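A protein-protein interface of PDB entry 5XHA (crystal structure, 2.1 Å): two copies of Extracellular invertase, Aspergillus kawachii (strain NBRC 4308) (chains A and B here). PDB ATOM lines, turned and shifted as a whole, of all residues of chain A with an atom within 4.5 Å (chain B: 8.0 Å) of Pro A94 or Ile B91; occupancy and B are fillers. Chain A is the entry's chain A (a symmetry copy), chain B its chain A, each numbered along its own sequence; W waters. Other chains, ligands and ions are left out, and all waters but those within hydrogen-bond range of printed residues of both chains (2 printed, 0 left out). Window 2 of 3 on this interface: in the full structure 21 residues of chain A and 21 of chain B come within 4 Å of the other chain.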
ATOM      1  N   GLY A  89      20.374 -20.796   2.504  1.00  0.00           N
ATOM      2  CA  GLY A  89      19.040 -21.108   2.970  1.00  0.00           C
ATOM      3  C   GLY A  89      18.998 -21.828   4.312  1.00  0.00           C
ATOM      4  O   GLY A  89      17.930 -22.213   4.759  1.00  0.00           O
ATOM      5  N   GLY A  90      20.151 -22.014   4.952  1.00  0.00           N
ATOM      6  CA  GLY A  90      20.215 -22.566   6.308  1.00  0.00           C
ATOM      7  C   GLY A  90      19.980 -21.512   7.376  1.00  0.00           C
ATOM      8  O   GLY A  90      19.768 -20.337   7.075  1.00  0.00           O
ATOM      9  N   ILE A  91      20.064 -21.927   8.630  1.00  0.00           N
ATOM     10  CA  ILE A  91      19.862 -21.020   9.768  1.00  0.00           C
ATOM     11  C   ILE A  91      20.979 -19.951   9.800  1.00  0.00           C
ATOM     12  O   ILE A  91      20.716 -18.777  10.077  1.00  0.00           O
ATOM     13  CB  ILE A  91      19.842 -21.810  11.102  1.00  0.00           C
ATOM     14  CG1 ILE A  91      18.647 -22.782  11.156  1.00  0.00           C
ATOM     15  CG2 ILE A  91      19.846 -20.891  12.322  1.00  0.00           C
ATOM     16  CD1 ILE A  91      17.289 -22.122  11.213  1.00  0.00           C
ATOM     17  N   ASN A  92      22.220 -20.358   9.512  1.00  0.00           N
ATOM     18  CA  ASN A  92      23.353 -19.418   9.592  1.00  0.00           C
ATOM     19  C   ASN A  92      23.569 -18.623   8.322  1.00  0.00           C
ATOM     20  O   ASN A  92      24.155 -17.522   8.372  1.00  0.00           O
ATOM     21  CB  ASN A  92      24.647 -20.137   9.939  1.00  0.00           C
ATOM     22  CG  ASN A  92      24.559 -20.943  11.233  1.00  0.00           C
ATOM     23  OD1 ASN A  92      23.674 -20.744  12.091  1.00  0.00           O
ATOM     24  ND2 ASN A  92      25.491 -21.871  11.375  1.00  0.00           N
ATOM     25  N   ASP A  93      23.105 -19.172   7.193  1.00  0.00           N
ATOM     26  CA  ASP A  93      23.352 -18.592   5.876  1.00  0.00           C
ATOM     27  C   ASP A  93      22.064 -18.451   5.058  1.00  0.00           C
ATOM     28  O   ASP A  93      21.995 -18.893   3.906  1.00  0.00           O
ATOM     29  CB  ASP A  93      24.411 -19.423   5.108  1.00  0.00           C
ATOM     30  CG  ASP A  93      24.103 -20.920   5.066  1.00  0.00           C
ATOM     31  OD1 ASP A  93      22.971 -21.345   5.420  1.00  0.00           O
ATOM     32  OD2 ASP A  93      24.998 -21.684   4.636  1.00  0.00           O
ATOM     33  N   PRO A  94      21.034 -17.820   5.649  1.00  0.00           N
ATOM     34  CA  PRO A  94      19.746 -17.764   4.975  1.00  0.00           C
ATOM     35  C   PRO A  94      19.781 -17.032   3.640  1.00  0.00           C
ATOM     36  O   PRO A  94      18.987 -17.342   2.764  1.00  0.00           O
ATOM     37  CB  PRO A  94      18.859 -17.019   5.977  1.00  0.00           C
ATOM     38  CG  PRO A  94      19.822 -16.164   6.748  1.00  0.00           C
ATOM     39  CD  PRO A  94      21.047 -17.015   6.877  1.00  0.00           C
ATOM     40  N   VAL A  95      20.713 -16.098   3.460  1.00  0.00           N
ATOM     41  CA  VAL A  95      20.741 -15.280   2.251  1.00  0.00           C
ATOM     42  C   VAL A  95      21.840 -15.693   1.269  1.00  0.00           C
ATOM     43  O   VAL A  95      21.612 -15.709   0.068  1.00  0.00           O
ATOM     44  CB  VAL A  95      20.832 -13.792   2.637  1.00  0.00           C
ATOM     45  CG1 VAL A  95      21.193 -12.914   1.452  1.00  0.00           C
ATOM     46  CG2 VAL A  95      19.506 -13.347   3.243  1.00  0.00           C
ATOM     47  N   ALA A  96      23.040 -16.008   1.741  1.00  0.00           N
ATOM     48  CA  ALA A  96      24.090 -16.359   0.793  1.00  0.00           C
ATOM     49  C   ALA A  96      25.198 -17.192   1.412  1.00  0.00           C
ATOM     50  O   ALA A  96      25.362 -17.225   2.637  1.00  0.00           O
ATOM     51  CB  ALA A  96      24.655 -15.101   0.136  1.00  0.00           C
ATOM     52  N   VAL A 118      26.179 -15.880   5.102  1.00  0.00           N
ATOM     53  CA  VAL A 118      25.613 -14.533   4.928  1.00  0.00           C
ATOM     54  C   VAL A 118      24.117 -14.470   5.287  1.00  0.00           C
ATOM     55  O   VAL A 118      23.292 -15.263   4.790  1.00  0.00           O
ATOM     56  CB  VAL A 118      25.788 -14.034   3.488  1.00  0.00           C
ATOM     57  CG1 VAL A 118      25.228 -12.620   3.312  1.00  0.00           C
ATOM     58  CG2 VAL A 118      27.258 -14.094   3.070  1.00  0.00           C
ATOM     59  N   SER A 119      23.787 -13.524   6.166  1.00  0.00           N
ATOM     60  CA  SER A 119      22.433 -13.352   6.681  1.00  0.00           C
ATOM     61  C   SER A 119      21.744 -12.035   6.275  1.00  0.00           C
ATOM     62  O   SER A 119      20.535 -11.896   6.463  1.00  0.00           O
ATOM     63  CB  SER A 119      22.481 -13.442   8.203  1.00  0.00           C
ATOM     64  OG  SER A 119      22.937 -14.721   8.606  1.00  0.00           O
ATOM     65  N   TYR A 120      22.510 -11.060   5.787  1.00  0.00           N
ATOM     66  CA  TYR A 120      21.978  -9.737   5.409  1.00  0.00           C
ATOM     67  C   TYR A 120      22.741  -9.205   4.204  1.00  0.00           C
ATOM     68  O   TYR A 120      23.962  -9.342   4.128  1.00  0.00           O
ATOM     69  CB  TYR A 120      22.062  -8.719   6.566  1.00  0.00           C
ATOM     70  CG  TYR A 120      21.261  -9.135   7.776  1.00  0.00           C
ATOM     71  CD1 TYR A 120      19.891  -8.845   7.876  1.00  0.00           C
ATOM     72  CD2 TYR A 120      21.847  -9.861   8.800  1.00  0.00           C
ATOM     73  CE1 TYR A 120      19.147  -9.285   8.965  1.00  0.00           C
ATOM     74  CE2 TYR A 120      21.115 -10.290   9.895  1.00  0.00           C
ATOM     75  CZ  TYR A 120      19.760 -10.007   9.970  1.00  0.00           C
ATOM     76  OH  TYR A 120      19.026 -10.427  11.068  1.00  0.00           O
ATOM     77  N   PRO B  88       8.650 -15.403  16.863  1.00  0.00           N
ATOM     78  CA  PRO B  88       9.794 -16.017  16.201  1.00  0.00           C
ATOM     79  C   PRO B  88       9.621 -16.141  14.689  1.00  0.00           C
ATOM     80  O   PRO B  88       8.568 -15.839  14.175  1.00  0.00           O
ATOM     81  CB  PRO B  88       9.853 -17.418  16.828  1.00  0.00           C
ATOM     82  CG  PRO B  88       8.450 -17.706  17.205  1.00  0.00           C
ATOM     83  CD  PRO B  88       7.911 -16.383  17.673  1.00  0.00           C
ATOM     84  N   GLY B  89      10.658 -16.600  14.006  1.00  0.00           N
ATOM     85  CA  GLY B  89      10.625 -16.806  12.575  1.00  0.00           C
ATOM     86  C   GLY B  89      11.438 -15.794  11.778  1.00  0.00           C
ATOM     87  O   GLY B  89      11.412 -15.824  10.558  1.00  0.00           O
ATOM     88  N   GLY B  90      12.153 -14.899  12.457  1.00  0.00           N
ATOM     89  CA  GLY B  90      13.078 -13.972  11.799  1.00  0.00           C
ATOM     90  C   GLY B  90      14.432 -14.602  11.522  1.00  0.00           C
ATOM     91  O   GLY B  90      14.670 -15.768  11.842  1.00  0.00           O
ATOM     92  N   ILE B  91      15.338 -13.812  10.967  1.00  0.00           N
ATOM     93  CA  ILE B  91      16.691 -14.283  10.642  1.00  0.00           C
ATOM     94  C   ILE B  91      17.454 -14.640  11.939  1.00  0.00           C
ATOM     95  O   ILE B  91      18.178 -15.639  11.986  1.00  0.00           O
ATOM     96  CB  ILE B  91      17.469 -13.206   9.844  1.00  0.00           C
ATOM     97  CG1 ILE B  91      16.806 -12.938   8.477  1.00  0.00           C
ATOM     98  CG2 ILE B  91      18.943 -13.564   9.668  1.00  0.00           C
ATOM     99  CD1 ILE B  91      16.864 -14.090   7.503  1.00  0.00           C
ATOM    100  N   ASN B  92      17.289 -13.824  12.986  1.00  0.00           N
ATOM    101  CA  ASN B  92      18.038 -14.050  14.235  1.00  0.00           C
ATOM    102  C   ASN B  92      17.360 -15.020  15.180  1.00  0.00           C
ATOM    103  O   ASN B  92      18.039 -15.642  16.023  1.00  0.00           O
ATOM    104  CB  ASN B  92      18.286 -12.747  14.977  1.00  0.00           C
ATOM    105  CG  ASN B  92      19.008 -11.700  14.132  1.00  0.00           C
ATOM    106  OD1 ASN B  92      19.644 -11.994  13.098  1.00  0.00           O
ATOM    107  ND2 ASN B  92      18.904 -10.458  14.575  1.00  0.00           N
ATOM    108  N   ASP B  93      16.035 -15.150  15.044  1.00  0.00           N
ATOM    109  CA  ASP B  93      15.223 -15.944  15.964  1.00  0.00           C
ATOM    110  C   ASP B  93      14.304 -16.921  15.222  1.00  0.00           C
ATOM    111  O   ASP B  93      13.095 -16.964  15.471  1.00  0.00           O
ATOM    112  CB  ASP B  93      14.410 -15.020  16.905  1.00  0.00           C
ATOM    113  CG  ASP B  93      13.616 -13.940  16.168  1.00  0.00           C
ATOM    114  OD1 ASP B  93      13.478 -13.997  14.917  1.00  0.00           O
ATOM    115  OD2 ASP B  93      13.088 -13.037  16.858  1.00  0.00           O
ATOM    116  N   PRO B  94      14.881 -17.725  14.310  1.00  0.00           N
ATOM    117  CA  PRO B  94      14.046 -18.584  13.486  1.00  0.00           C
ATOM    118  C   PRO B  94      13.243 -19.609  14.278  1.00  0.00           C
ATOM    119  O   PRO B  94      12.174 -20.005  13.838  1.00  0.00           O
ATOM    120  CB  PRO B  94      15.059 -19.283  12.573  1.00  0.00           C
ATOM    121  CG  PRO B  94      16.326 -19.292  13.376  1.00  0.00           C
ATOM    122  CD  PRO B  94      16.311 -17.982  14.102  1.00  0.00           C
ATOM    123  N   VAL B  95      13.723 -20.007  15.454  1.00  0.00           N
ATOM    124  CA  VAL B  95      13.067 -21.064  16.221  1.00  0.00           C
ATOM    125  C   VAL B  95      12.270 -20.536  17.417  1.00  0.00           C
ATOM    126  O   VAL B  95      11.181 -21.019  17.686  1.00  0.00           O
ATOM    127  CB  VAL B  95      14.105 -22.123  16.633  1.00  0.00           C
ATOM    128  CG1 VAL B  95      13.570 -23.068  17.694  1.00  0.00           C
ATOM    129  CG2 VAL B  95      14.544 -22.905  15.400  1.00  0.00           C
ATOM    130  N   TYR B 115      16.333  -8.844  23.704  1.00  0.00           N
ATOM    131  CA  TYR B 115      15.719 -10.128  23.993  1.00  0.00           C
ATOM    132  C   TYR B 115      16.536 -11.277  23.463  1.00  0.00           C
ATOM    133  O   TYR B 115      17.363 -11.104  22.573  1.00  0.00           O
ATOM    134  CB  TYR B 115      14.313 -10.170  23.389  1.00  0.00           C
ATOM    135  CG  TYR B 115      14.263 -10.361  21.879  1.00  0.00           C
ATOM    136  CD1 TYR B 115      14.396  -9.286  21.024  1.00  0.00           C
ATOM    137  CD2 TYR B 115      14.058 -11.635  21.316  1.00  0.00           C
ATOM    138  CE1 TYR B 115      14.332  -9.448  19.653  1.00  0.00           C
ATOM    139  CE2 TYR B 115      14.002 -11.807  19.947  1.00  0.00           C
ATOM    140  CZ  TYR B 115      14.136 -10.716  19.123  1.00  0.00           C
ATOM    141  OH  TYR B 115      14.074 -10.876  17.762  1.00  0.00           O
ATOM    142  N   SER B 117      17.064 -14.134  21.179  1.00  0.00           N
ATOM    143  CA  SER B 117      16.701 -14.706  19.895  1.00  0.00           C
ATOM    144  C   SER B 117      17.296 -16.126  19.782  1.00  0.00           C
ATOM    145  O   SER B 117      18.518 -16.280  19.865  1.00  0.00           O
ATOM    146  CB  SER B 117      17.234 -13.814  18.780  1.00  0.00           C
ATOM    147  OG  SER B 117      18.514 -13.276  19.093  1.00  0.00           O
ATOM    148  N   VAL B 118      16.425 -17.129  19.582  1.00  0.00           N
ATOM    149  CA  VAL B 118      16.774 -18.558  19.603  1.00  0.00           C
ATOM    150  C   VAL B 118      16.786 -19.183  18.196  1.00  0.00           C
ATOM    151  O   VAL B 118      15.813 -19.072  17.422  1.00  0.00           O
ATOM    152  CB  VAL B 118      15.804 -19.359  20.482  1.00  0.00           C
ATOM    153  CG1 VAL B 118      16.183 -20.841  20.529  1.00  0.00           C
ATOM    154  CG2 VAL B 118      15.737 -18.767  21.890  1.00  0.00           C
ATOM    155  N   SER B 119      17.907 -19.829  17.875  1.00  0.00           N
ATOM    156  CA  SER B 119      18.135 -20.429  16.565  1.00  0.00           C
ATOM    157  C   SER B 119      18.243 -21.965  16.560  1.00  0.00           C
ATOM    158  O   SER B 119      18.206 -22.577  15.493  1.00  0.00           O
ATOM    159  CB  SER B 119      19.412 -19.836  15.979  1.00  0.00           C
ATOM    160  OG  SER B 119      19.268 -18.439  15.797  1.00  0.00           O
ATOM    161  N   THR B 135      21.198 -15.939  21.198  1.00  0.00           N
ATOM    162  CA  THR B 135      21.849 -14.641  20.980  1.00  0.00           C
ATOM    163  C   THR B 135      20.925 -13.578  21.529  1.00  0.00           C
ATOM    164  O   THR B 135      19.796 -13.882  21.903  1.00  0.00           O
ATOM    165  CB  THR B 135      22.095 -14.361  19.498  1.00  0.00           C
ATOM    166  OG1 THR B 135      20.844 -14.390  18.795  1.00  0.00           O
ATOM    167  CG2 THR B 135      23.047 -15.392  18.899  1.00  0.00           C
ATOM    168  N   SER B 137      19.167  -9.916  20.649  1.00  0.00           N
ATOM    169  CA  SER B 137      18.823  -9.073  19.516  1.00  0.00           C
ATOM    170  C   SER B 137      17.970  -7.879  19.957  1.00  0.00           C
ATOM    171  O   SER B 137      17.379  -7.886  21.050  1.00  0.00           O
ATOM    172  CB  SER B 137      18.068  -9.910  18.475  1.00  0.00           C
ATOM    173  OG  SER B 137      18.920 -10.877  17.868  1.00  0.00           O
ATOM    174  N   LYS B 150      11.664  -5.910  14.730  1.00  0.00           N
ATOM    175  CA  LYS B 150      13.056  -6.350  14.788  1.00  0.00           C
ATOM    176  C   LYS B 150      13.937  -5.454  13.949  1.00  0.00           C
ATOM    177  O   LYS B 150      13.608  -5.177  12.807  1.00  0.00           O
ATOM    178  CB  LYS B 150      13.176  -7.773  14.293  1.00  0.00           C
ATOM    179  CG  LYS B 150      12.447  -8.750  15.186  1.00  0.00           C
ATOM    180  CD  LYS B 150      12.291 -10.104  14.535  1.00  0.00           C
ATOM    181  CE  LYS B 150      11.260 -10.936  15.247  1.00  0.00           C
ATOM    182  NZ  LYS B 150      11.177 -12.291  14.657  1.00  0.00           N
ATOM    183  N   LEU B 151      15.052  -4.990  14.504  1.00  0.00           N
ATOM    184  CA  LEU B 151      16.036  -4.310  13.669  1.00  0.00           C
ATOM    185  C   LEU B 151      16.516  -5.311  12.631  1.00  0.00           C
ATOM    186  O   LEU B 151      16.719  -6.503  12.943  1.00  0.00           O
ATOM    187  CB  LEU B 151      17.238  -3.779  14.474  1.00  0.00           C
ATOM    188  CG  LEU B 151      16.946  -2.746  15.565  1.00  0.00           C
ATOM    189  CD1 LEU B 151      18.262  -2.135  16.024  1.00  0.00           C
ATOM    190  CD2 LEU B 151      15.987  -1.658  15.087  1.00  0.00           C
ATOM    191  N   ASP B 152      16.701  -4.816  11.406  1.00  0.00           N
ATOM    192  CA  ASP B 152      17.100  -5.630  10.271  1.00  0.00           C
ATOM    193  C   ASP B 152      18.636  -5.785  10.262  1.00  0.00           C
ATOM    194  O   ASP B 152      19.346  -5.257   9.415  1.00  0.00           O
ATOM    195  CB  ASP B 152      16.563  -4.961   9.000  1.00  0.00           C
ATOM    196  CG  ASP B 152      16.708  -5.819   7.780  1.00  0.00           C
ATOM    197  OD1 ASP B 152      16.797  -7.054   7.903  1.00  0.00           O
ATOM    198  OD2 ASP B 152      16.740  -5.249   6.677  1.00  0.00           O
ATOM    199  N   GLN B 153      19.133  -6.502  11.250  1.00  0.00           N
ATOM    200  CA  GLN B 153      20.554  -6.723  11.430  1.00  0.00           C
ATOM    201  C   GLN B 153      20.696  -7.917  12.378  1.00  0.00           C
ATOM    202  O   GLN B 153      19.709  -8.360  12.946  1.00  0.00           O
ATOM    203  CB  GLN B 153      21.228  -5.489  12.030  1.00  0.00           C
ATOM    204  CG  GLN B 153      20.675  -5.126  13.411  1.00  0.00           C
ATOM    205  CD  GLN B 153      21.652  -4.319  14.213  1.00  0.00           C
ATOM    206  OE1 GLN B 153      21.854  -3.156  13.960  1.00  0.00           O
ATOM    207  NE2 GLN B 153      22.299  -4.953  15.155  1.00  0.00           N
ATOM    208  N   GLY B 154      21.914  -8.436  12.525  1.00  0.00           N
ATOM    209  CA  GLY B 154      22.182  -9.534  13.433  1.00  0.00           C
ATOM    210  C   GLY B 154      22.082  -9.172  14.907  1.00  0.00           C
ATOM    211  O   GLY B 154      21.864  -8.018  15.264  1.00  0.00           O
ATOM    212  N   PRO B 155      22.260 -10.170  15.779  1.00  0.00           N
ATOM    213  CA  PRO B 155      22.216  -9.881  17.196  1.00  0.00           C
ATOM    214  C   PRO B 155      23.307  -8.911  17.613  1.00  0.00           C
ATOM    215  O   PRO B 155      24.399  -8.918  17.030  1.00  0.00           O
ATOM    216  CB  PRO B 155      22.456 -11.247  17.859  1.00  0.00           C
ATOM    217  CG  PRO B 155      23.096 -12.078  16.810  1.00  0.00           C
ATOM    218  CD  PRO B 155      22.521 -11.594  15.504  1.00  0.00           C
HETATM  219  O   HOH W   1      18.136 -17.706  10.106  1.00  0.00           O
HETATM  220  O   HOH W   2      16.770  -9.137  11.771  1.00  0.00           O
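The backbone carbonyl oxygen of Gln B153 is in hydrogen-bond range of the side-chain hydroxyl of Tyr A120.
The side-chain hydroxyl of Tyr A120 lies within hydrogen-bond range of the side-chain amide oxygen of Asn B92 (2.6 Å).
Among the printed residues, merely in contact across the chains: Ile A91 with Pro B94 (3.7 Å), Ile A91 with Ser B119 (3.8 Å), Pro A94 with Ile B91 (3.7 Å), Ser A119 with Ile B91 (3.8 Å), Tyr A120 with Ile B91 (3.4 Å), Tyr A120 with Asp B152 (3.4 Å) and Tyr A120 with Gly B154 (3.3 Å).
Hydrophobic or aromatic side chains of chain B that line the printed part of chain A: Ile B91 and Pro B94.
Hydrophobic or aromatic side chains of chain A that line the printed part of chain B: Ile A91, Pro A94 and Tyr A120.
Along chain A the printed residues that touch a printed residue of chain B span positions 91 to 120.
Among the printed residues, 9 pairs touch across the chains.
Among the printed residues, no Asp or Glu carboxylate lies within 4 Å of a Lys or Arg side-chain nitrogen of the other chain.
Ile A91 touches Pro B94, and with the chains exchanged Pro A94 touches Ile B91.
Ile A91 touches Ser B119, and with the chains exchanged Ser A119 touches Ile B91.
9 positions are printed for both chains.
The backbone carbonyl oxygen (O) of Asn A92 sits at hydrogen-bond distance from the side-chain hydroxyl (OG) of Ser A119, 3.1 Å away.
The side-chain hydroxyl (OG) of Ser B119 is in hydrogen-bond range of the backbone carbonyl oxygen (O) of Asn B92, 3.1 Å away.
The backbone carbonyl oxygen (O) of Gln B153 sits at hydrogen-bond distance from the side-chain amide nitrogen (ND2) of Asn B92 (2.8 Å).
The side-chain hydroxyl (OG) of Ser B137 is in hydrogen-bond range of the side-chain amide nitrogen (ND2) of Asn B92, 3.3 Å away.
Pro A94 touches just one residue of chain B: Ile B91 (3.7 Å).
Of chain A, only Pro A94, Ser A119 and Tyr A120 come within 4 Å of Ile B91.
Of the printed residues of chain A, Pro B94 touches Ile A91 (3.7 Å).
Of the printed residues of chain A, Asn B92 touches Tyr A120.
Of the printed residues of chain A, Asp B152 touches Tyr A120 (3.4 Å).
Of the printed residues of chain A, Gly B154 touches Tyr A120.
Printed residues of chain A within 4 Å of Ser B119: Ile A91.
Asn A92 touches none of the printed residues of chain B.
The nearest printed residue of chain A that does not touch Ile B91 is Ile A91 (4.5 Å).
The nearest printed residue of chain A that does not touch Pro B94 is Asn A92 (7.1 Å).
Water W2 lies within hydrogen-bond range of OH of Tyr A120 (2.7 Å), O of Leu B151 (2.9 Å) and O of Gln B153 (3.3 Å).
Water W1 lies within hydrogen-bond range of the backbone carbonyl oxygen of Ile A91 (2.8 Å) and the backbone carbonyl oxygen of Ile B91 (2.8 Å).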
